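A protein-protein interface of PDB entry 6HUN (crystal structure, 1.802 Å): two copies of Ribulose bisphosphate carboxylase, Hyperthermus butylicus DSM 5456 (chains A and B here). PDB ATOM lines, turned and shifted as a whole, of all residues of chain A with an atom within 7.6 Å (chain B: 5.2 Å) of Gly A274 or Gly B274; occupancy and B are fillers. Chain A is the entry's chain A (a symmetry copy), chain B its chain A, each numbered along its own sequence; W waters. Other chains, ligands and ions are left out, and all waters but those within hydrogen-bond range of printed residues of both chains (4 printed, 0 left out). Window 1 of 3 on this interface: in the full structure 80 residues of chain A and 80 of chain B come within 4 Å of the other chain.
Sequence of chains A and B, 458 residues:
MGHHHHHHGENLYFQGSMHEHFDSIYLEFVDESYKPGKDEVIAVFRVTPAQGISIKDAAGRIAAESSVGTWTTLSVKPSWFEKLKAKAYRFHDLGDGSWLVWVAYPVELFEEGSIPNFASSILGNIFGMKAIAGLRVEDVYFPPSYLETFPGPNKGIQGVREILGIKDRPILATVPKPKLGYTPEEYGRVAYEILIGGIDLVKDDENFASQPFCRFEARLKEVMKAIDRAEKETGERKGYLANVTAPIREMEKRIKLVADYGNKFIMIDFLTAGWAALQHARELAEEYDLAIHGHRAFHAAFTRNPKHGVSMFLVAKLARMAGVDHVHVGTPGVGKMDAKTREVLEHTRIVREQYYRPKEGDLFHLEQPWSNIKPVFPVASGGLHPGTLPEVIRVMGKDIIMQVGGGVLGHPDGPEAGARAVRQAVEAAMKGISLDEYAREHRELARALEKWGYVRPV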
ATOM      1  N   ILE A 115      24.828  13.712   4.063  1.00  0.00           N
ATOM      2  CA  ILE A 115      25.123  15.145   4.066  1.00  0.00           C
ATOM      3  C   ILE A 115      24.234  15.882   5.062  1.00  0.00           C
ATOM      4  O   ILE A 115      24.725  16.814   5.733  1.00  0.00           O
ATOM      5  CB  ILE A 115      25.023  15.715   2.642  1.00  0.00           C
ATOM      6  CG1 ILE A 115      25.989  15.001   1.691  1.00  0.00           C
ATOM      7  CG2 ILE A 115      25.275  17.230   2.678  1.00  0.00           C
ATOM      8  CD1 ILE A 115      27.445  15.386   1.911  1.00  0.00           C
ATOM      9  N   PRO A 116      22.939  15.575   5.187  1.00  0.00           N
ATOM     10  CA  PRO A 116      22.141  16.266   6.198  1.00  0.00           C
ATOM     11  C   PRO A 116      22.714  16.155   7.589  1.00  0.00           C
ATOM     12  O   PRO A 116      22.672  17.150   8.332  1.00  0.00           O
ATOM     13  CB  PRO A 116      20.772  15.574   6.100  1.00  0.00           C
ATOM     14  CG  PRO A 116      20.717  15.207   4.607  1.00  0.00           C
ATOM     15  CD  PRO A 116      22.099  14.680   4.360  1.00  0.00           C
ATOM     16  N   THR A 245      13.887  19.277 -10.488  1.00  0.00           N
ATOM     17  CA  THR A 245      13.639  19.892  -9.181  1.00  0.00           C
ATOM     18  C   THR A 245      12.142  19.846  -8.865  1.00  0.00           C
ATOM     19  O   THR A 245      11.313  20.394  -9.598  1.00  0.00           O
ATOM     20  CB  THR A 245      14.191  21.322  -9.187  1.00  0.00           C
ATOM     21  OG1 THR A 245      15.638  21.312  -9.454  1.00  0.00           O
ATOM     22  CG2 THR A 245      13.949  22.036  -7.798  1.00  0.00           C
ATOM     23  N   ALA A 246      11.805  19.235  -7.704  1.00  0.00           N
ATOM     24  CA  ALA A 246      10.399  18.905  -7.441  1.00  0.00           C
ATOM     25  C   ALA A 246      10.294  18.258  -6.067  1.00  0.00           C
ATOM     26  O   ALA A 246      11.312  17.833  -5.495  1.00  0.00           O
ATOM     27  CB  ALA A 246       9.856  17.974  -8.519  1.00  0.00           C
ATOM     28  N   ILE A 248       9.756  15.142  -3.692  1.00  0.00           N
ATOM     29  CA  ILE A 248      10.456  13.863  -3.918  1.00  0.00           C
ATOM     30  C   ILE A 248       9.659  12.944  -4.862  1.00  0.00           C
ATOM     31  O   ILE A 248      10.203  12.417  -5.851  1.00  0.00           O
ATOM     32  CB  ILE A 248      10.760  13.175  -2.560  1.00  0.00           C
ATOM     33  CG1 ILE A 248      11.802  13.976  -1.706  1.00  0.00           C
ATOM     34  CG2 ILE A 248      11.166  11.683  -2.727  1.00  0.00           C
ATOM     35  CD1 ILE A 248      13.258  14.261  -2.354  1.00  0.00           C
ATOM     36  N   MET A 251       9.824  14.266  -8.324  1.00  0.00           N
ATOM     37  CA  MET A 251      11.176  14.145  -8.898  1.00  0.00           C
ATOM     38  C   MET A 251      11.444  12.713  -9.348  1.00  0.00           C
ATOM     39  O   MET A 251      12.027  12.470 -10.434  1.00  0.00           O
ATOM     40  CB  MET A 251      12.224  14.563  -7.861  1.00  0.00           C
ATOM     41  CG  MET A 251      13.689  14.397  -8.382  1.00  0.00           C
ATOM     42  SD  MET A 251      14.901  14.774  -7.117  1.00  0.00           S
ATOM     43  CE  MET A 251      14.814  13.311  -6.116  1.00  0.00           C
ATOM     44  N   ILE A 268      19.306  19.206 -11.086  1.00  0.00           N
ATOM     45  CA  ILE A 268      18.624  19.417  -9.803  1.00  0.00           C
ATOM     46  C   ILE A 268      19.202  20.656  -9.123  1.00  0.00           C
ATOM     47  O   ILE A 268      20.420  20.910  -9.163  1.00  0.00           O
ATOM     48  CB  ILE A 268      18.706  18.200  -8.895  1.00  0.00           C
ATOM     49  CG1 ILE A 268      17.884  18.488  -7.616  1.00  0.00           C
ATOM     50  CG2 ILE A 268      20.160  17.887  -8.482  1.00  0.00           C
ATOM     51  CD1 ILE A 268      17.562  17.241  -6.896  1.00  0.00           C
ATOM     52  N   ASP A 269      18.297  21.485  -8.622  1.00  0.00           N
ATOM     53  CA  ASP A 269      18.693  22.673  -7.843  1.00  0.00           C
ATOM     54  C   ASP A 269      18.966  22.136  -6.462  1.00  0.00           C
ATOM     55  O   ASP A 269      18.067  21.978  -5.653  1.00  0.00           O
ATOM     56  CB  ASP A 269      17.585  23.704  -7.844  1.00  0.00           C
ATOM     57  CG  ASP A 269      17.169  24.187  -9.232  1.00  0.00           C
ATOM     58  OD1 ASP A 269      17.748  23.854 -10.299  1.00  0.00           O
ATOM     59  OD2 ASP A 269      16.216  24.986  -9.265  1.00  0.00           O
ATOM     60  N   PHE A 270      20.232  21.810  -6.156  1.00  0.00           N
ATOM     61  CA  PHE A 270      20.412  20.985  -4.964  1.00  0.00           C
ATOM     62  C   PHE A 270      20.298  21.778  -3.658  1.00  0.00           C
ATOM     63  O   PHE A 270      20.257  21.158  -2.598  1.00  0.00           O
ATOM     64  CB  PHE A 270      21.762  20.244  -5.039  1.00  0.00           C
ATOM     65  CG  PHE A 270      22.993  21.158  -5.141  1.00  0.00           C
ATOM     66  CD1 PHE A 270      23.687  21.549  -3.995  1.00  0.00           C
ATOM     67  CD2 PHE A 270      23.491  21.540  -6.390  1.00  0.00           C
ATOM     68  CE1 PHE A 270      24.821  22.332  -4.100  1.00  0.00           C
ATOM     69  CE2 PHE A 270      24.622  22.372  -6.531  1.00  0.00           C
ATOM     70  CZ  PHE A 270      25.301  22.730  -5.402  1.00  0.00           C
ATOM     71  N   LEU A 271      20.354  23.109  -3.704  1.00  0.00           N
ATOM     72  CA  LEU A 271      20.169  23.870  -2.455  1.00  0.00           C
ATOM     73  C   LEU A 271      18.715  24.212  -2.233  1.00  0.00           C
ATOM     74  O   LEU A 271      18.289  24.280  -1.062  1.00  0.00           O
ATOM     75  CB  LEU A 271      21.025  25.165  -2.458  1.00  0.00           C
ATOM     76  CG  LEU A 271      22.521  24.749  -2.466  1.00  0.00           C
ATOM     77  CD1 LEU A 271      23.289  26.080  -2.704  1.00  0.00           C
ATOM     78  CD2 LEU A 271      22.961  23.988  -1.232  1.00  0.00           C
ATOM     79  N   THR A 272      17.909  24.349  -3.290  1.00  0.00           N
ATOM     80  CA  THR A 272      16.480  24.636  -3.066  1.00  0.00           C
ATOM     81  C   THR A 272      15.633  23.371  -2.911  1.00  0.00           C
ATOM     82  O   THR A 272      14.668  23.393  -2.113  1.00  0.00           O
ATOM     83  CB  THR A 272      15.924  25.497  -4.224  1.00  0.00           C
ATOM     84  OG1 THR A 272      15.925  24.763  -5.452  1.00  0.00           O
ATOM     85  CG2 THR A 272      16.747  26.794  -4.406  1.00  0.00           C
ATOM     86  N   ALA A 273      15.973  22.282  -3.607  1.00  0.00           N
ATOM     87  CA  ALA A 273      15.361  20.987  -3.272  1.00  0.00           C
ATOM     88  C   ALA A 273      15.984  20.413  -2.002  1.00  0.00           C
ATOM     89  O   ALA A 273      15.293  19.847  -1.143  1.00  0.00           O
ATOM     90  CB  ALA A 273      15.518  20.012  -4.466  1.00  0.00           C
ATOM     91  N   GLY A 274      17.283  20.579  -1.825  1.00  0.00           N
ATOM     92  CA  GLY A 274      17.950  20.220  -0.597  1.00  0.00           C
ATOM     93  C   GLY A 274      18.914  19.033  -0.773  1.00  0.00           C
ATOM     94  O   GLY A 274      18.892  18.319  -1.773  1.00  0.00           O
ATOM     95  N   TRP A 275      19.827  18.908   0.186  1.00  0.00           N
ATOM     96  CA  TRP A 275      20.860  17.867   0.106  1.00  0.00           C
ATOM     97  C   TRP A 275      20.261  16.478   0.074  1.00  0.00           C
ATOM     98  O   TRP A 275      20.764  15.617  -0.638  1.00  0.00           O
ATOM     99  CB  TRP A 275      21.805  17.967   1.295  1.00  0.00           C
ATOM    100  CG  TRP A 275      22.659  19.212   1.187  1.00  0.00           C
ATOM    101  CD1 TRP A 275      22.594  20.307   2.004  1.00  0.00           C
ATOM    102  CD2 TRP A 275      23.708  19.442   0.271  1.00  0.00           C
ATOM    103  NE1 TRP A 275      23.569  21.238   1.605  1.00  0.00           N
ATOM    104  CE2 TRP A 275      24.252  20.726   0.549  1.00  0.00           C
ATOM    105  CE3 TRP A 275      24.276  18.675  -0.761  1.00  0.00           C
ATOM    106  CZ2 TRP A 275      25.376  21.261  -0.171  1.00  0.00           C
ATOM    107  CZ3 TRP A 275      25.373  19.241  -1.516  1.00  0.00           C
ATOM    108  CH2 TRP A 275      25.873  20.507  -1.198  1.00  0.00           C
ATOM    109  N   ALA A 276      19.208  16.222   0.860  1.00  0.00           N
ATOM    110  CA  ALA A 276      18.662  14.870   0.814  1.00  0.00           C
ATOM    111  C   ALA A 276      18.094  14.576  -0.569  1.00  0.00           C
ATOM    112  O   ALA A 276      18.218  13.438  -1.084  1.00  0.00           O
ATOM    113  CB  ALA A 276      17.597  14.675   1.950  1.00  0.00           C
ATOM    114  N   ALA A 277      17.461  15.557  -1.193  1.00  0.00           N
ATOM    115  CA  ALA A 277      16.956  15.350  -2.562  1.00  0.00           C
ATOM    116  C   ALA A 277      18.092  15.036  -3.517  1.00  0.00           C
ATOM    117  O   ALA A 277      17.953  14.180  -4.429  1.00  0.00           O
ATOM    118  CB  ALA A 277      16.237  16.617  -3.080  1.00  0.00           C
ATOM    119  N   LEU A 278      19.206  15.749  -3.377  1.00  0.00           N
ATOM    120  CA  LEU A 278      20.346  15.475  -4.273  1.00  0.00           C
ATOM    121  C   LEU A 278      20.857  14.063  -4.054  1.00  0.00           C
ATOM    122  O   LEU A 278      21.096  13.318  -5.024  1.00  0.00           O
ATOM    123  CB  LEU A 278      21.462  16.498  -4.029  1.00  0.00           C
ATOM    124  CG  LEU A 278      22.791  16.194  -4.720  1.00  0.00           C
ATOM    125  CD1 LEU A 278      22.613  16.060  -6.308  1.00  0.00           C
ATOM    126  CD2 LEU A 278      23.850  17.311  -4.358  1.00  0.00           C
ATOM    127  N   GLN A 279      21.018  13.647  -2.767  1.00  0.00           N
ATOM    128  CA  GLN A 279      21.534  12.286  -2.553  1.00  0.00           C
ATOM    129  C   GLN A 279      20.554  11.232  -3.062  1.00  0.00           C
ATOM    130  O   GLN A 279      20.982  10.155  -3.514  1.00  0.00           O
ATOM    131  CB  GLN A 279      21.847  12.019  -1.056  1.00  0.00           C
ATOM    132  CG  GLN A 279      22.990  12.985  -0.569  1.00  0.00           C
ATOM    133  CD  GLN A 279      23.597  12.509   0.726  1.00  0.00           C
ATOM    134  OE1 GLN A 279      23.178  12.919   1.816  1.00  0.00           O
ATOM    135  NE2 GLN A 279      24.554  11.561   0.614  1.00  0.00           N
ATOM    136  N   HIS A 280      19.239  11.487  -2.925  1.00  0.00           N
ATOM    137  CA  HIS A 280      18.241  10.577  -3.501  1.00  0.00           C
ATOM    138  C   HIS A 280      18.324  10.547  -5.030  1.00  0.00           C
ATOM    139  O   HIS A 280      18.268   9.464  -5.646  1.00  0.00           O
ATOM    140  CB  HIS A 280      16.847  11.021  -3.075  1.00  0.00           C
ATOM    141  CG  HIS A 280      15.771   9.998  -3.358  1.00  0.00           C
ATOM    142  ND1 HIS A 280      15.861   8.679  -2.960  1.00  0.00           N
ATOM    143  CD2 HIS A 280      14.574  10.122  -3.972  1.00  0.00           C
ATOM    144  CE1 HIS A 280      14.777   8.026  -3.346  1.00  0.00           C
ATOM    145  NE2 HIS A 280      13.984   8.880  -3.974  1.00  0.00           N
ATOM    146  N   ASP B 269      15.333  18.252  10.438  1.00  0.00           N
ATOM    147  CA  ASP B 269      16.120  19.486  10.254  1.00  0.00           C
ATOM    148  C   ASP B 269      15.799  19.924   8.849  1.00  0.00           C
ATOM    149  O   ASP B 269      16.398  19.468   7.890  1.00  0.00           O
ATOM    150  CB  ASP B 269      17.597  19.209  10.441  1.00  0.00           C
ATOM    151  CG  ASP B 269      17.966  18.632  11.805  1.00  0.00           C
ATOM    152  OD1 ASP B 269      17.153  18.484  12.754  1.00  0.00           O
ATOM    153  OD2 ASP B 269      19.164  18.334  11.961  1.00  0.00           O
ATOM    154  N   PHE B 270      14.809  20.815   8.682  1.00  0.00           N
ATOM    155  CA  PHE B 270      14.295  20.956   7.322  1.00  0.00           C
ATOM    156  C   PHE B 270      15.204  21.792   6.415  1.00  0.00           C
ATOM    157  O   PHE B 270      14.960  21.827   5.213  1.00  0.00           O
ATOM    158  CB  PHE B 270      12.869  21.542   7.359  1.00  0.00           C
ATOM    159  CG  PHE B 270      12.759  22.923   8.024  1.00  0.00           C
ATOM    160  CD1 PHE B 270      12.826  24.090   7.260  1.00  0.00           C
ATOM    161  CD2 PHE B 270      12.501  23.031   9.393  1.00  0.00           C
ATOM    162  CE1 PHE B 270      12.678  25.325   7.861  1.00  0.00           C
ATOM    163  CE2 PHE B 270      12.384  24.278  10.045  1.00  0.00           C
ATOM    164  CZ  PHE B 270      12.432  25.409   9.282  1.00  0.00           C
ATOM    165  N   LEU B 271      16.161  22.535   6.971  1.00  0.00           N
ATOM    166  CA  LEU B 271      17.082  23.279   6.092  1.00  0.00           C
ATOM    167  C   LEU B 271      18.300  22.455   5.751  1.00  0.00           C
ATOM    168  O   LEU B 271      18.836  22.614   4.636  1.00  0.00           O
ATOM    169  CB  LEU B 271      17.513  24.621   6.742  1.00  0.00           C
ATOM    170  CG  LEU B 271      16.252  25.519   6.868  1.00  0.00           C
ATOM    171  CD1 LEU B 271      16.722  26.725   7.729  1.00  0.00           C
ATOM    172  CD2 LEU B 271      15.629  25.905   5.543  1.00  0.00           C
ATOM    173  N   THR B 272      18.718  21.523   6.613  1.00  0.00           N
ATOM    174  CA  THR B 272      19.879  20.687   6.254  1.00  0.00           C
ATOM    175  C   THR B 272      19.492  19.427   5.479  1.00  0.00           C
ATOM    176  O   THR B 272      20.266  19.015   4.585  1.00  0.00           O
ATOM    177  CB  THR B 272      20.664  20.296   7.527  1.00  0.00           C
ATOM    178  OG1 THR B 272      19.884  19.437   8.364  1.00  0.00           O
ATOM    179  CG2 THR B 272      21.085  21.547   8.335  1.00  0.00           C
ATOM    180  N   ALA B 273      18.329  18.831   5.761  1.00  0.00           N
ATOM    181  CA  ALA B 273      17.805  17.798   4.855  1.00  0.00           C
ATOM    182  C   ALA B 273      17.214  18.437   3.600  1.00  0.00           C
ATOM    183  O   ALA B 273      17.384  17.936   2.480  1.00  0.00           O
ATOM    184  CB  ALA B 273      16.751  16.938   5.598  1.00  0.00           C
ATOM    185  N   GLY B 274      16.549  19.570   3.742  1.00  0.00           N
ATOM    186  CA  GLY B 274      16.084  20.343   2.616  1.00  0.00           C
ATOM    187  C   GLY B 274      14.549  20.360   2.505  1.00  0.00           C
ATOM    188  O   GLY B 274      13.841  19.580   3.138  1.00  0.00           O
ATOM    189  N   TRP B 275      14.054  21.342   1.756  1.00  0.00           N
ATOM    190  CA  TRP B 275      12.603  21.526   1.626  1.00  0.00           C
ATOM    191  C   TRP B 275      11.931  20.314   1.020  1.00  0.00           C
ATOM    192  O   TRP B 275      10.834  19.958   1.433  1.00  0.00           O
ATOM    193  CB  TRP B 275      12.300  22.740   0.760  1.00  0.00           C
ATOM    194  CG  TRP B 275      12.675  24.014   1.486  1.00  0.00           C
ATOM    195  CD1 TRP B 275      13.691  24.865   1.147  1.00  0.00           C
ATOM    196  CD2 TRP B 275      12.015  24.581   2.598  1.00  0.00           C
ATOM    197  NE1 TRP B 275      13.701  25.950   2.041  1.00  0.00           N
ATOM    198  CE2 TRP B 275      12.688  25.788   2.932  1.00  0.00           C
ATOM    199  CE3 TRP B 275      10.888  24.204   3.349  1.00  0.00           C
ATOM    200  CZ2 TRP B 275      12.247  26.650   3.994  1.00  0.00           C
ATOM    201  CZ3 TRP B 275      10.481  25.048   4.450  1.00  0.00           C
ATOM    202  CH2 TRP B 275      11.175  26.228   4.733  1.00  0.00           C
ATOM    203  N   ALA B 276      12.550  19.681   0.015  1.00  0.00           N
ATOM    204  CA  ALA B 276      11.870  18.523  -0.556  1.00  0.00           C
ATOM    205  C   ALA B 276      11.753  17.414   0.484  1.00  0.00           C
ATOM    206  O   ALA B 276      10.724  16.698   0.543  1.00  0.00           O
ATOM    207  CB  ALA B 276      12.607  18.046  -1.856  1.00  0.00           C
ATOM    208  N   ALA B 277      12.776  17.232   1.304  1.00  0.00           N
ATOM    209  CA  ALA B 277      12.687  16.223   2.374  1.00  0.00           C
ATOM    210  C   ALA B 277      11.556  16.546   3.331  1.00  0.00           C
ATOM    211  O   ALA B 277      10.832  15.635   3.809  1.00  0.00           O
ATOM    212  CB  ALA B 277      14.000  16.170   3.190  1.00  0.00           C
ATOM    213  N   LEU B 278      11.413  17.821   3.680  1.00  0.00           N
ATOM    214  CA  LEU B 278      10.320  18.193   4.600  1.00  0.00           C
ATOM    215  C   LEU B 278       8.976  17.897   3.961  1.00  0.00           C
ATOM    216  O   LEU B 278       8.085  17.308   4.603  1.00  0.00           O
ATOM    217  CB  LEU B 278      10.429  19.676   4.970  1.00  0.00           C
ATOM    218  CG  LEU B 278       9.231  20.251   5.728  1.00  0.00           C
ATOM    219  CD1 LEU B 278       8.950  19.444   7.085  1.00  0.00           C
ATOM    220  CD2 LEU B 278       9.468  21.787   6.018  1.00  0.00           C
HETATM  221  O   HOH W   1      19.434  20.964   2.257  1.00  0.00           O
HETATM  222  O   HOH W   2       9.047  16.346  -1.284  1.00  0.00           O
HETATM  223  O   HOH W   3      15.676  17.535   0.335  1.00  0.00           O
HETATM  224  O   HOH W   4      16.231  22.939   0.583  1.00  0.00           O
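Water W2 bridges O of Ala B276 and N of Ile A248.
Water W3 lies within hydrogen-bond range of O of Ala B273 (2.8 Å), O of Ala A273 (2.8 Å), N of Ala A277 (3.1 Å) and N of Ala B277 (3.1 Å).
Water W4 lies within hydrogen-bond range of N of Trp B275, O of Leu A271 and O of Thr A272.
Water W1 lies within hydrogen-bond range of the backbone NH (N) of Trp A275 (2.9 Å), the backbone carbonyl oxygen (O) of Leu B271 (3.0 Å) and the backbone carbonyl oxygen (O) of Thr B272 (3.1 Å).
Thr A272 touches Trp B275, and with the chains exchanged Trp A275 touches Thr B272.
Ala A273 touches Gly B274, and with the chains exchanged Gly A274 touches Ala B273.
Ala A273 touches Trp B275, and with the chains exchanged Trp A275 touches Ala B273.
Gly B274 touches its own counterpart, Gly A274.
Along chain A the printed residues that touch a printed residue of chain B span positions 116 to 276.
Of the 10 printed residues of chain B, 5 touch a printed residue of chain A.
Hydrophobic or aromatic side chains of chain B within 4 Å of the printed part of chain A: Trp B275 and Ala B276.
Among the printed residues, 13 pairs touch across the chains.
Among the printed residues, no Asp or Glu carboxylate lies within 4 Å of a Lys or Arg side-chain nitrogen of the other chain.
Pro A116 touches Thr B272.
Pro A116 touches Ala B273.
Ala A246 touches Ala B276.
Ile A248 touches Ala B276.
O of Thr A272 touches CD1 of Trp B275, at 3.7 Å.
Gly B274 touches Ala A273.
C of Gly A274 touches O of Ala B273, at 3.8 Å.
Gly B274 touches Gly A274 (CA to CA, 3.7 Å).
Trp A275 touches Thr B272.
Of the printed residues of chain B, Pro A116 touches Thr B272 (3.6 Å) and Ala B273 (3.9 Å).
Gly A274 touches just these residues of chain B: Ala B273 (3.8 Å) and Gly B274 (3.7 Å).
Of the printed residues of chain B, Trp A275 touches Thr B272 (3.7 Å) and Ala B273 (3.5 Å).
Of the printed residues of chain A, Thr B272 touches Pro A116 (3.6 Å) and Trp A275 (3.7 Å).
Of chain A, only Pro A116, Gly A274, Trp A275 and Ala A276 come within 4 Å of Ala B273.
Of chain A, only Ala A273 and Gly A274 come within 4 Å of Gly B274.
The nearest residue of chain B that does not touch Gly A274 is Trp B275 (4.7 Å).
The nearest residue of chain A that does not touch Gly B274 is Trp A275 (4.7 Å).
The backbone carbonyl oxygen (O) of Ala A273 sits at hydrogen-bond distance from the backbone NH (N) of Ala B276 (3.0 Å).
The backbone NH (N) of Trp B275 sits at hydrogen-bond distance from the backbone carbonyl oxygen (O) of Ala A273 (3.5 Å).
O of Ala B273 lies within hydrogen-bond range of N of Trp A275.
The backbone carbonyl oxygen (O) of Ala B273 lies within hydrogen-bond range of the backbone NH (N) of Ala A276, at 3.0 Å.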
